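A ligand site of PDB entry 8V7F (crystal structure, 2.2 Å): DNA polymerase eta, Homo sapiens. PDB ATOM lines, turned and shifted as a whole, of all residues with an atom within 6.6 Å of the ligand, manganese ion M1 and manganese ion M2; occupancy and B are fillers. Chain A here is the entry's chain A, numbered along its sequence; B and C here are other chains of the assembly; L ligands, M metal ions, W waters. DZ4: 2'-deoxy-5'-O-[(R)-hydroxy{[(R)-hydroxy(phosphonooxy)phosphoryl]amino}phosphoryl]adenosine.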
ATOM      1  N   ASP A  16      35.979  11.211  -6.577  1.00  0.00           N
ATOM      2  CA  ASP A  16      35.130  12.375  -6.776  1.00  0.00           C
ATOM      3  C   ASP A  16      34.091  12.093  -7.863  1.00  0.00           C
ATOM      4  O   ASP A  16      34.452  11.711  -8.984  1.00  0.00           O
ATOM      5  CB  ASP A  16      35.972  13.596  -7.158  1.00  0.00           C
ATOM      6  CG  ASP A  16      35.164  14.867  -7.244  1.00  0.00           C
ATOM      7  OD1 ASP A  16      34.458  15.054  -8.258  1.00  0.00           O
ATOM      8  OD2 ASP A  16      35.213  15.684  -6.296  1.00  0.00           O
ATOM      9  N   MET A  17      32.815  12.286  -7.519  1.00  0.00           N
ATOM     10  CA  MET A  17      31.706  12.024  -8.450  1.00  0.00           C
ATOM     11  C   MET A  17      31.742  12.963  -9.652  1.00  0.00           C
ATOM     12  O   MET A  17      32.050  14.150  -9.521  1.00  0.00           O
ATOM     13  CB  MET A  17      30.369  12.193  -7.730  1.00  0.00           C
ATOM     14  CG  MET A  17      30.048  11.213  -6.602  1.00  0.00           C
ATOM     15  SD  MET A  17      30.955   9.645  -6.634  1.00  0.00           S
ATOM     16  CE  MET A  17      29.736   8.623  -7.461  1.00  0.00           C
ATOM     17  N   ASP A  18      31.403  12.427 -10.822  1.00  0.00           N
ATOM     18  CA  ASP A  18      31.303  13.241 -12.029  1.00  0.00           C
ATOM     19  C   ASP A  18      29.980  13.994 -12.059  1.00  0.00           C
ATOM     20  O   ASP A  18      28.930  13.386 -11.815  1.00  0.00           O
ATOM     21  CB  ASP A  18      31.449  12.376 -13.277  1.00  0.00           C
ATOM     22  CG  ASP A  18      32.772  11.645 -13.327  1.00  0.00           C
ATOM     23  OD1 ASP A  18      33.747  12.126 -12.712  1.00  0.00           O
ATOM     24  OD2 ASP A  18      32.861  10.605 -14.010  1.00  0.00           O
ATOM     25  N   CYS A  19      30.038  15.286 -12.390  1.00  0.00           N
ATOM     26  CA  CYS A  19      28.918  16.236 -12.367  1.00  0.00           C
ATOM     27  C   CYS A  19      27.797  15.782 -11.435  1.00  0.00           C
ATOM     28  O   CYS A  19      26.697  15.480 -11.888  1.00  0.00           O
ATOM     29  CB  CYS A  19      28.375  16.454 -13.790  1.00  0.00           C
ATOM     30  SG  CYS A  19      27.967  14.962 -14.782  1.00  0.00           S
ATOM     31  N   PHE A  20      28.082  15.780 -10.119  1.00  0.00           N
ATOM     32  CA  PHE A  20      27.324  14.967  -9.166  1.00  0.00           C
ATOM     33  C   PHE A  20      25.842  15.299  -9.143  1.00  0.00           C
ATOM     34  O   PHE A  20      24.991  14.411  -9.277  1.00  0.00           O
ATOM     35  CB  PHE A  20      27.915  15.136  -7.757  1.00  0.00           C
ATOM     36  CG  PHE A  20      27.256  14.258  -6.728  1.00  0.00           C
ATOM     37  CD1 PHE A  20      26.973  12.929  -7.009  1.00  0.00           C
ATOM     38  CD2 PHE A  20      26.873  14.772  -5.497  1.00  0.00           C
ATOM     39  CE1 PHE A  20      26.344  12.113  -6.069  1.00  0.00           C
ATOM     40  CE2 PHE A  20      26.250  13.961  -4.553  1.00  0.00           C
ATOM     41  CZ  PHE A  20      25.989  12.626  -4.836  1.00  0.00           C
ATOM     42  N   PHE A  21      25.490  16.571  -8.919  1.00  0.00           N
ATOM     43  CA  PHE A  21      24.074  16.914  -8.826  1.00  0.00           C
ATOM     44  C   PHE A  21      23.337  16.589 -10.131  1.00  0.00           C
ATOM     45  O   PHE A  21      22.181  16.143 -10.115  1.00  0.00           O
ATOM     46  CB  PHE A  21      23.897  18.392  -8.466  1.00  0.00           C
ATOM     47  CG  PHE A  21      24.255  18.746  -7.039  1.00  0.00           C
ATOM     48  CD1 PHE A  21      25.089  17.943  -6.281  1.00  0.00           C
ATOM     49  CD2 PHE A  21      23.751  19.913  -6.461  1.00  0.00           C
ATOM     50  CE1 PHE A  21      25.407  18.288  -4.969  1.00  0.00           C
ATOM     51  CE2 PHE A  21      24.068  20.258  -5.148  1.00  0.00           C
ATOM     52  CZ  PHE A  21      24.897  19.442  -4.410  1.00  0.00           C
ATOM     53  N   VAL A  22      24.019  16.785 -11.267  1.00  0.00           N
ATOM     54  CA  VAL A  22      23.437  16.446 -12.565  1.00  0.00           C
ATOM     55  C   VAL A  22      23.179  14.942 -12.656  1.00  0.00           C
ATOM     56  O   VAL A  22      22.123  14.514 -13.143  1.00  0.00           O
ATOM     57  CB  VAL A  22      24.350  16.933 -13.707  1.00  0.00           C
ATOM     58  CG1 VAL A  22      23.931  16.328 -15.030  1.00  0.00           C
ATOM     59  CG2 VAL A  22      24.332  18.451 -13.785  1.00  0.00           C
ATOM     60  N   GLN A  41      19.748  26.713  -9.011  1.00  0.00           N
ATOM     61  CA  GLN A  41      19.067  27.138  -7.790  1.00  0.00           C
ATOM     62  C   GLN A  41      18.262  28.398  -8.080  1.00  0.00           C
ATOM     63  O   GLN A  41      18.811  29.359  -8.640  1.00  0.00           O
ATOM     64  CB  GLN A  41      20.029  27.446  -6.637  1.00  0.00           C
ATOM     65  CG  GLN A  41      20.842  26.301  -6.093  1.00  0.00           C
ATOM     66  CD  GLN A  41      21.728  26.743  -4.939  1.00  0.00           C
ATOM     67  OE1 GLN A  41      21.832  26.058  -3.924  1.00  0.00           O
ATOM     68  NE2 GLN A  41      22.380  27.893  -5.100  1.00  0.00           N
ATOM     69  N   ILE A  50      23.464  28.585 -11.872  1.00  0.00           N
ATOM     70  CA  ILE A  50      23.830  27.211 -12.189  1.00  0.00           C
ATOM     71  C   ILE A  50      24.850  26.724 -11.159  1.00  0.00           C
ATOM     72  O   ILE A  50      25.810  27.424 -10.835  1.00  0.00           O
ATOM     73  CB  ILE A  50      24.384  27.106 -13.618  1.00  0.00           C
ATOM     74  CG1 ILE A  50      23.259  27.266 -14.628  1.00  0.00           C
ATOM     75  CG2 ILE A  50      25.075  25.759 -13.831  1.00  0.00           C
ATOM     76  CD1 ILE A  50      23.729  27.379 -16.041  1.00  0.00           C
ATOM     77  N   ILE A  51      24.630  25.514 -10.656  1.00  0.00           N
ATOM     78  CA  ILE A  51      25.556  24.919  -9.698  1.00  0.00           C
ATOM     79  C   ILE A  51      26.127  23.586 -10.170  1.00  0.00           C
ATOM     80  O   ILE A  51      27.138  23.146  -9.602  1.00  0.00           O
ATOM     81  CB  ILE A  51      24.917  24.762  -8.303  1.00  0.00           C
ATOM     82  CG1 ILE A  51      23.681  23.856  -8.332  1.00  0.00           C
ATOM     83  CG2 ILE A  51      24.556  26.124  -7.714  1.00  0.00           C
ATOM     84  CD1 ILE A  51      23.175  23.492  -6.953  1.00  0.00           C
ATOM     85  N   ALA A  52      25.553  22.942 -11.182  1.00  0.00           N
ATOM     86  CA  ALA A  52      26.240  21.768 -11.736  1.00  0.00           C
ATOM     87  C   ALA A  52      25.962  21.638 -13.233  1.00  0.00           C
ATOM     88  O   ALA A  52      24.891  22.006 -13.697  1.00  0.00           O
ATOM     89  CB  ALA A  52      25.837  20.469 -11.022  1.00  0.00           C
ATOM     90  N   VAL A  53      26.948  21.114 -13.971  1.00  0.00           N
ATOM     91  CA  VAL A  53      26.924  21.122 -15.434  1.00  0.00           C
ATOM     92  C   VAL A  53      27.409  19.785 -15.974  1.00  0.00           C
ATOM     93  O   VAL A  53      28.510  19.335 -15.636  1.00  0.00           O
ATOM     94  CB  VAL A  53      27.796  22.260 -16.012  1.00  0.00           C
ATOM     95  CG1 VAL A  53      27.557  22.385 -17.507  1.00  0.00           C
ATOM     96  CG2 VAL A  53      27.484  23.571 -15.331  1.00  0.00           C
ATOM     97  N   TYR A  55      28.906  17.151 -18.820  1.00  0.00           N
ATOM     98  CA  TYR A  55      30.049  17.336 -19.710  1.00  0.00           C
ATOM     99  C   TYR A  55      29.607  17.685 -21.127  1.00  0.00           C
ATOM    100  O   TYR A  55      30.293  18.452 -21.824  1.00  0.00           O
ATOM    101  CB  TYR A  55      30.946  16.106 -19.661  1.00  0.00           C
ATOM    102  CG  TYR A  55      31.774  16.054 -18.394  1.00  0.00           C
ATOM    103  CD1 TYR A  55      31.226  15.571 -17.205  1.00  0.00           C
ATOM    104  CD2 TYR A  55      33.077  16.541 -18.372  1.00  0.00           C
ATOM    105  CE1 TYR A  55      31.984  15.543 -16.024  1.00  0.00           C
ATOM    106  CE2 TYR A  55      33.828  16.529 -17.206  1.00  0.00           C
ATOM    107  CZ  TYR A  55      33.283  16.026 -16.039  1.00  0.00           C
ATOM    108  OH  TYR A  55      34.027  16.008 -14.877  1.00  0.00           O
ATOM    109  N   ARG A  58      29.158  21.294 -20.858  1.00  0.00           N
ATOM    110  CA  ARG A  58      30.463  21.955 -20.757  1.00  0.00           C
ATOM    111  C   ARG A  58      31.093  22.126 -22.133  1.00  0.00           C
ATOM    112  O   ARG A  58      31.785  23.130 -22.365  1.00  0.00           O
ATOM    113  CB  ARG A  58      31.397  21.177 -19.836  1.00  0.00           C
ATOM    114  CG  ARG A  58      30.919  21.095 -18.405  1.00  0.00           C
ATOM    115  CD  ARG A  58      31.863  20.301 -17.527  1.00  0.00           C
ATOM    116  NE  ARG A  58      31.200  19.862 -16.311  1.00  0.00           N
ATOM    117  CZ  ARG A  58      31.820  19.399 -15.234  1.00  0.00           C
ATOM    118  NH1 ARG A  58      33.140  19.321 -15.169  1.00  0.00           N
ATOM    119  NH2 ARG A  58      31.087  18.993 -14.191  1.00  0.00           N
ATOM    120  N   ARG A  64      29.627  26.422 -13.859  1.00  0.00           N
ATOM    121  CA  ARG A  64      29.025  26.753 -12.582  1.00  0.00           C
ATOM    122  C   ARG A  64      29.155  28.251 -12.320  1.00  0.00           C
ATOM    123  O   ARG A  64      30.077  28.905 -12.806  1.00  0.00           O
ATOM    124  CB  ARG A  64      29.686  25.928 -11.458  1.00  0.00           C
ATOM    125  CG  ARG A  64      29.862  26.638 -10.107  1.00  0.00           C
ATOM    126  CD  ARG A  64      30.632  25.784  -9.095  1.00  0.00           C
ATOM    127  NE  ARG A  64      32.081  25.886  -9.261  1.00  0.00           N
ATOM    128  CZ  ARG A  64      32.866  24.856  -9.536  1.00  0.00           C
ATOM    129  NH1 ARG A  64      32.386  23.626  -9.661  1.00  0.00           N
ATOM    130  NH2 ARG A  64      34.174  25.066  -9.699  1.00  0.00           N
ATOM    131  N   LEU A  92      18.962  21.007  -0.032  1.00  0.00           N
ATOM    132  CA  LEU A  92      19.897  20.119  -0.710  1.00  0.00           C
ATOM    133  C   LEU A  92      19.784  18.671  -0.254  1.00  0.00           C
ATOM    134  O   LEU A  92      20.718  17.891  -0.485  1.00  0.00           O
ATOM    135  CB  LEU A  92      21.334  20.618  -0.517  1.00  0.00           C
ATOM    136  CG  LEU A  92      21.598  22.081  -0.903  1.00  0.00           C
ATOM    137  CD1 LEU A  92      22.999  22.486  -0.467  1.00  0.00           C
ATOM    138  CD2 LEU A  92      21.415  22.286  -2.393  1.00  0.00           C
ATOM    139  N   SER A 116      34.086  16.188   0.811  1.00  0.00           N
ATOM    140  CA  SER A 116      32.990  17.058   0.383  1.00  0.00           C
ATOM    141  C   SER A 116      31.784  16.186   0.086  1.00  0.00           C
ATOM    142  O   SER A 116      31.888  14.957   0.039  1.00  0.00           O
ATOM    143  CB  SER A 116      33.382  17.883  -0.854  1.00  0.00           C
ATOM    144  OG  SER A 116      33.001  17.196  -2.047  1.00  0.00           O
ATOM    145  N   ILE A 117      30.659  16.851  -0.187  1.00  0.00           N
ATOM    146  CA  ILE A 117      29.395  16.164  -0.439  1.00  0.00           C
ATOM    147  C   ILE A 117      29.560  15.099  -1.524  1.00  0.00           C
ATOM    148  O   ILE A 117      28.800  14.130  -1.568  1.00  0.00           O
ATOM    149  CB  ILE A 117      28.275  17.149  -0.826  1.00  0.00           C
ATOM    150  CG1 ILE A 117      26.906  16.486  -0.677  1.00  0.00           C
ATOM    151  CG2 ILE A 117      28.446  17.642  -2.253  1.00  0.00           C
ATOM    152  CD1 ILE A 117      25.754  17.483  -0.595  1.00  0.00           C
ATOM    153  N   ASP A 118      30.552  15.259  -2.396  1.00  0.00           N
ATOM    154  CA  ASP A 118      30.700  14.314  -3.505  1.00  0.00           C
ATOM    155  C   ASP A 118      32.097  13.701  -3.584  1.00  0.00           C
ATOM    156  O   ASP A 118      32.435  13.106  -4.622  1.00  0.00           O
ATOM    157  CB  ASP A 118      30.353  14.964  -4.842  1.00  0.00           C
ATOM    158  CG  ASP A 118      31.556  15.594  -5.536  1.00  0.00           C
ATOM    159  OD1 ASP A 118      32.344  16.298  -4.865  1.00  0.00           O
ATOM    160  OD2 ASP A 118      31.700  15.359  -6.753  1.00  0.00           O
ATOM    161  N   GLU A 119      32.911  13.805  -2.541  1.00  0.00           N
ATOM    162  CA  GLU A 119      34.234  13.201  -2.656  1.00  0.00           C
ATOM    163  C   GLU A 119      34.773  12.786  -1.303  1.00  0.00           C
ATOM    164  O   GLU A 119      34.450  13.381  -0.264  1.00  0.00           O
ATOM    165  CB  GLU A 119      35.241  14.136  -3.352  1.00  0.00           C
ATOM    166  CG  GLU A 119      35.765  15.271  -2.512  1.00  0.00           C
ATOM    167  CD  GLU A 119      36.029  16.503  -3.359  1.00  0.00           C
ATOM    168  OE1 GLU A 119      35.053  17.191  -3.720  1.00  0.00           O
ATOM    169  OE2 GLU A 119      37.208  16.760  -3.668  1.00  0.00           O
ATOM    170  N   SER A 216      35.281   9.662 -10.909  1.00  0.00           N
ATOM    171  CA  SER A 216      36.699   9.607 -11.228  1.00  0.00           C
ATOM    172  C   SER A 216      37.502   9.436  -9.940  1.00  0.00           C
ATOM    173  O   SER A 216      36.970   9.611  -8.841  1.00  0.00           O
ATOM    174  CB  SER A 216      37.141  10.860 -11.988  1.00  0.00           C
ATOM    175  OG  SER A 216      36.467  10.963 -13.222  1.00  0.00           O
ATOM    176  N   LYS A 227      44.196  14.027  -5.169  1.00  0.00           N
ATOM    177  CA  LYS A 227      43.202  14.956  -5.705  1.00  0.00           C
ATOM    178  C   LYS A 227      43.644  15.538  -7.055  1.00  0.00           C
ATOM    179  O   LYS A 227      42.854  15.603  -8.020  1.00  0.00           O
ATOM    180  CB  LYS A 227      42.943  16.065  -4.673  1.00  0.00           C
ATOM    181  CG  LYS A 227      42.045  17.201  -5.137  1.00  0.00           C
ATOM    182  CD  LYS A 227      40.610  16.734  -5.357  1.00  0.00           C
ATOM    183  CE  LYS A 227      39.679  17.902  -5.596  1.00  0.00           C
ATOM    184  NZ  LYS A 227      38.274  17.509  -5.898  1.00  0.00           N
ATOM    185  N   LYS A 234      39.240  13.331 -15.858  1.00  0.00           N
ATOM    186  CA  LYS A 234      37.797  13.345 -15.751  1.00  0.00           C
ATOM    187  C   LYS A 234      37.157  13.463 -17.135  1.00  0.00           C
ATOM    188  O   LYS A 234      37.695  14.130 -18.020  1.00  0.00           O
ATOM    189  CB  LYS A 234      37.345  14.508 -14.867  1.00  0.00           C
ATOM    190  CG  LYS A 234      37.413  14.218 -13.380  1.00  0.00           C
ATOM    191  CD  LYS A 234      36.413  15.069 -12.614  1.00  0.00           C
ATOM    192  CE  LYS A 234      36.154  14.492 -11.232  1.00  0.00           C
ATOM    193  NZ  LYS A 234      34.693  14.218 -11.039  1.00  0.00           N
ATOM    194  N   PRO A 235      35.983  12.830 -17.347  1.00  0.00           N
ATOM    195  CA  PRO A 235      35.205  12.021 -16.416  1.00  0.00           C
ATOM    196  C   PRO A 235      35.347  10.511 -16.625  1.00  0.00           C
ATOM    197  O   PRO A 235      35.876  10.065 -17.639  1.00  0.00           O
ATOM    198  CB  PRO A 235      33.768  12.468 -16.729  1.00  0.00           C
ATOM    199  CG  PRO A 235      33.799  12.622 -18.229  1.00  0.00           C
ATOM    200  CD  PRO A 235      35.203  13.140 -18.563  1.00  0.00           C
ATOM    201  P    DT B   4      24.527  35.525  -4.839  1.00  0.00           P
ATOM    202  OP1  DT B   4      23.315  36.377  -4.905  1.00  0.00           O
ATOM    203  OP2  DT B   4      25.699  35.960  -4.046  1.00  0.00           O
ATOM    204  O5'  DT B   4      24.097  34.077  -4.320  1.00  0.00           O
ATOM    205  C5'  DT B   4      22.910  33.479  -4.803  1.00  0.00           C
ATOM    206  C4'  DT B   4      22.691  32.112  -4.171  1.00  0.00           C
ATOM    207  O4'  DT B   4      23.750  31.200  -4.560  1.00  0.00           O
ATOM    208  C3'  DT B   4      22.659  32.088  -2.641  1.00  0.00           C
ATOM    209  O3'  DT B   4      21.655  31.181  -2.231  1.00  0.00           O
ATOM    210  C2'  DT B   4      24.063  31.582  -2.285  1.00  0.00           C
ATOM    211  C1'  DT B   4      24.312  30.604  -3.416  1.00  0.00           C
ATOM    212  N1   DT B   4      25.761  30.318  -3.716  1.00  0.00           N
ATOM    213  C2   DT B   4      26.137  29.025  -3.974  1.00  0.00           C
ATOM    214  O2   DT B   4      25.363  28.081  -3.935  1.00  0.00           O
ATOM    215  N3   DT B   4      27.452  28.858  -4.275  1.00  0.00           N
ATOM    216  C4   DT B   4      28.427  29.825  -4.340  1.00  0.00           C
ATOM    217  O4   DT B   4      29.591  29.569  -4.626  1.00  0.00           O
ATOM    218  C5   DT B   4      27.974  31.172  -4.082  1.00  0.00           C
ATOM    219  C7   DT B   4      28.949  32.320  -4.121  1.00  0.00           C
ATOM    220  C6   DT B   4      26.673  31.356  -3.780  1.00  0.00           C
ATOM    221  P    DG B   5      21.293  30.985  -0.681  1.00  0.00           P
ATOM    222  OP1  DG B   5      19.830  30.770  -0.617  1.00  0.00           O
ATOM    223  OP2  DG B   5      21.891  32.086   0.111  1.00  0.00           O
ATOM    224  O5'  DG B   5      22.004  29.607  -0.307  1.00  0.00           O
ATOM    225  C5'  DG B   5      21.631  28.418  -1.002  1.00  0.00           C
ATOM    226  C4'  DG B   5      22.450  27.237  -0.537  1.00  0.00           C
ATOM    227  O4'  DG B   5      23.809  27.340  -1.061  1.00  0.00           O
ATOM    228  C3'  DG B   5      22.595  27.117   0.987  1.00  0.00           C
ATOM    229  O3'  DG B   5      22.476  25.761   1.368  1.00  0.00           O
ATOM    230  C2'  DG B   5      24.007  27.656   1.236  1.00  0.00           C
ATOM    231  C1'  DG B   5      24.725  27.170  -0.006  1.00  0.00           C
ATOM    232  N9   DG B   5      25.951  27.910  -0.296  1.00  0.00           N
ATOM    233  C8   DG B   5      26.160  29.263  -0.147  1.00  0.00           C
ATOM    234  N7   DG B   5      27.372  29.639  -0.489  1.00  0.00           N
ATOM    235  C5   DG B   5      28.001  28.464  -0.875  1.00  0.00           C
ATOM    236  C6   DG B   5      29.323  28.236  -1.340  1.00  0.00           C
ATOM    237  O6   DG B   5      30.227  29.056  -1.509  1.00  0.00           O
ATOM    238  N1   DG B   5      29.545  26.891  -1.630  1.00  0.00           N
ATOM    239  C2   DG B   5      28.619  25.895  -1.485  1.00  0.00           C
ATOM    240  N2   DG B   5      29.016  24.659  -1.812  1.00  0.00           N
ATOM    241  N3   DG B   5      27.378  26.084  -1.047  1.00  0.00           N
ATOM    242  C4   DG B   5      27.134  27.389  -0.759  1.00  0.00           C
ATOM    243  P   CAR C   8      38.581  22.771  -5.369  1.00  0.00           P
ATOM    244  OP1 CAR C   8      38.267  21.356  -5.785  1.00  0.00           O
ATOM    245  OP2 CAR C   8      39.982  23.163  -5.754  1.00  0.00           O
ATOM    246  O5' CAR C   8      37.492  23.844  -6.004  1.00  0.00           O
ATOM    247  C5' CAR C   8      36.268  23.399  -6.529  1.00  0.00           C
ATOM    248  C4' CAR C   8      35.475  22.836  -5.304  1.00  0.00           C
ATOM    249  O4' CAR C   8      35.363  23.925  -4.340  1.00  0.00           O
ATOM    250  C3' CAR C   8      34.059  22.353  -5.579  1.00  0.00           C
ATOM    251  O3' CAR C   8      33.758  21.258  -4.702  1.00  0.00           O
ATOM    252  C2' CAR C   8      33.217  23.556  -5.197  1.00  0.00           C
ATOM    253  O2' CAR C   8      33.088  24.531  -6.206  1.00  0.00           O
ATOM    254  C1' CAR C   8      34.002  24.102  -4.002  1.00  0.00           C
ATOM    255  N1  CAR C   8      33.747  25.498  -3.731  1.00  0.00           N
ATOM    256  C2  CAR C   8      32.648  25.883  -2.945  1.00  0.00           C
ATOM    257  O2  CAR C   8      31.898  25.019  -2.509  1.00  0.00           O
ATOM    258  N3  CAR C   8      32.414  27.196  -2.686  1.00  0.00           N
ATOM    259  C4  CAR C   8      33.219  28.148  -3.170  1.00  0.00           C
ATOM    260  N4  CAR C   8      32.977  29.433  -2.905  1.00  0.00           N
ATOM    261  C5  CAR C   8      34.339  27.774  -3.960  1.00  0.00           C
ATOM    262  C6  CAR C   8      34.588  26.477  -4.219  1.00  0.00           C
HETATM  263  N1  DZ4 L   1      28.013  26.216  -4.806  1.00  0.00           N
HETATM  264  C2  DZ4 L   1      27.042  25.324  -4.616  1.00  0.00           C
HETATM  265  N3  DZ4 L   1      27.110  24.045  -4.917  1.00  0.00           N
HETATM  266  C4  DZ4 L   1      28.265  23.593  -5.458  1.00  0.00           C
HETATM  267  C5  DZ4 L   1      29.323  24.475  -5.681  1.00  0.00           C
HETATM  268  C6  DZ4 L   1      29.182  25.811  -5.341  1.00  0.00           C
HETATM  269  N6  DZ4 L   1      30.169  26.696  -5.546  1.00  0.00           N
HETATM  270  N7  DZ4 L   1      30.328  23.771  -6.233  1.00  0.00           N
HETATM  271  C8  DZ4 L   1      29.938  22.476  -6.341  1.00  0.00           C
HETATM  272  N9  DZ4 L   1      28.684  22.378  -5.875  1.00  0.00           N
HETATM  273  PA  DZ4 L   1      32.373  19.333  -7.771  1.00  0.00           P
HETATM  274  PB  DZ4 L   1      30.934  18.355 -10.080  1.00  0.00           P
HETATM  275  PG  DZ4 L   1      33.171  17.363 -11.733  1.00  0.00           P
HETATM  276  C1' DZ4 L   1      27.900  21.103  -5.845  1.00  0.00           C
HETATM  277  O1A DZ4 L   1      32.993  18.021  -7.656  1.00  0.00           O
HETATM  278  O1B DZ4 L   1      30.759  17.128  -9.292  1.00  0.00           O
HETATM  279  O1G DZ4 L   1      34.049  18.373 -12.397  1.00  0.00           O
HETATM  280  C2' DZ4 L   1      27.408  20.693  -7.212  1.00  0.00           C
HETATM  281  O2A DZ4 L   1      33.431  20.438  -7.548  1.00  0.00           O
HETATM  282  O2B DZ4 L   1      29.543  18.907 -10.502  1.00  0.00           O
HETATM  283  O2G DZ4 L   1      33.791  16.868 -10.419  1.00  0.00           O
HETATM  284  C3' DZ4 L   1      28.400  19.633  -7.660  1.00  0.00           C
HETATM  285  O3' DZ4 L   1      27.729  18.693  -8.493  1.00  0.00           O
HETATM  286  N3A DZ4 L   1      31.751  19.528  -9.272  1.00  0.00           N
HETATM  287  O3B DZ4 L   1      31.712  18.050 -11.419  1.00  0.00           O
HETATM  288  O3G DZ4 L   1      32.924  16.158 -12.659  1.00  0.00           O
HETATM  289  C4' DZ4 L   1      28.833  18.997  -6.342  1.00  0.00           C
HETATM  290  O4' DZ4 L   1      28.709  20.049  -5.330  1.00  0.00           O
HETATM  291  C5' DZ4 L   1      30.286  18.454  -6.397  1.00  0.00           C
HETATM  292  O5' DZ4 L   1      31.213  19.511  -6.634  1.00  0.00           O
HETATM  293 MN    MN M   1      32.673  16.085  -8.656  1.00  0.00          MN
HETATM  294 MN    MN M   2      34.117  17.421  -5.694  1.00  0.00          MN
HETATM  295  O   HOH W   1      30.364  22.147  -9.784  1.00  0.00           O
HETATM  296  O   HOH W   2      35.685  18.685  -6.751  1.00  0.00           O
HETATM  297  O   HOH W   3      29.365  20.565 -12.349  1.00  0.00           O
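Manganese ion M2 is bound by OD2 of Asp 16 (2.1 Å), OE1 of Glu 119 (2.2 Å), OD1 of Asp 118 (2.3 Å), water W2 (2.3 Å) and O1A of the ligand (2.3 Å).
OH of Tyr 55 lies within hydrogen-bond range of O3G of the ligand, 2.5 Å away.
A nitrogen (N6) of the ligand lies within hydrogen-bond range of O4 of DT 4 of chain B, at 3.1 Å.
O2A of the ligand sits close to O3' of CAR 8 of chain C (3.0 Å).
The side-chain amino group of Lys 234 is in salt-bridge range of an oxygen (O3G) of the ligand, 3.1 Å away.
The guanidinium group of Arg 58 is in salt-bridge range of an oxygen (O1G) of the ligand.
O3G of the ligand sits at hydrogen-bond distance from N of Cys 19.
The backbone NH of Phe 20 sits at hydrogen-bond distance from an oxygen (O3') of the ligand, at 3.4 Å.
An oxygen (O3') of the ligand sits at hydrogen-bond distance from the backbone NH (N) of Phe 21 (3.1 Å).
O2A of the ligand is in salt-bridge range of NH1 of Arg 64, 3.96 Å away.
Ser 116 touches manganese ion M2.
CAR 8 of chain C touches manganese ion M2 (O3' to MN, 3.98 Å).
Five residues have an atom within 4 Å of manganese ion M2: Asp 16, Ser 116, Asp 118, Glu 119 and CAR 8 of chain C.
The nearest printed residue that does not touch manganese ion M2 is Lys 227 (4.2 Å).
Water W2 bridges an oxygen (O2A) of the ligand and the side-chain amino group of Lys 227.
Water W3 lies within hydrogen-bond range of O2B of the ligand, N of Val 53 and NH2 of Arg 58.
Water W1 lies within hydrogen-bond range of the guanidinium group (NH1) of Arg 64 (2.5 Å), a nitrogen (N3A) of the ligand (3.0 Å) and the backbone carbonyl oxygen (O) of Ile 51 (3.4 Å).
OD1 of Asp 16 binds manganese ion M1 (2.1 Å).
An oxygen (O1A) of the ligand binds manganese ion M1.
O of Met 17 binds manganese ion M1 (2.2 Å).
O2G of the ligand is bound to manganese ion M1 (2.2 Å).
OD2 of Asp 118 is bound to manganese ion M1, at 2.3 Å.
An oxygen (O1B) of the ligand is bound to manganese ion M1.
Manganese ion M1 has six donor atoms within binding distance.
Merely in contact with the ligand: Asp 18 (3.4 Å), Ile 51 (3.4 Å), Ala 52 (3.6 Å), Ile 117 (3.9 Å) and DG 5 of chain B (3.4 Å).
Within 4 Å of the ligand: Asp 16, Met 17, Asp 18, Cys 19, Phe 20, Phe 21, Ile 51, Ala 52, Tyr 55, Arg 58, Arg 64, Ile 117, Asp 118, Lys 234, DT 4 of chain B, DG 5 of chain B and CAR 8 of chain C.
Along chain A the residues within 4 Å of the ligand span positions 16 to 234.
The backbone carbonyl oxygen (O) of Asp 16 sits at hydrogen-bond distance from the side-chain amino group (NZ) of Lys 234 (3.3 Å).
O of Asp 16 lies within hydrogen-bond range of N of Ser 216 (2.9 Å).
O of Met 17 lies close to NZ of Lys 234 (3.0 Å).
NH1 of Arg 58 lies close to OH of Tyr 55 (3.4 Å).
O2 of DT 4 of chain B is in hydrogen-bond range of the side-chain amide nitrogen (NE2) of Gln 41 (3.2 Å).
OP1 of CAR 8 of chain C lies within salt-bridge range of NZ of Lys 227 (3.8 Å).
The side-chain carboxylate (OD1) of Asp 18 is in salt-bridge range of the side-chain amino group (NZ) of Lys 234, 2.8 Å away.
The backbone carbonyl oxygen (O) of Val 53 sits at hydrogen-bond distance from the guanidinium group (NE) of Arg 58, 2.8 Å away.
Merely in contact with manganese ion M1: Lys 234.
Four residues have an atom within 4 Å of manganese ion M1: Asp 16, Met 17, Asp 118 and Lys 234.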
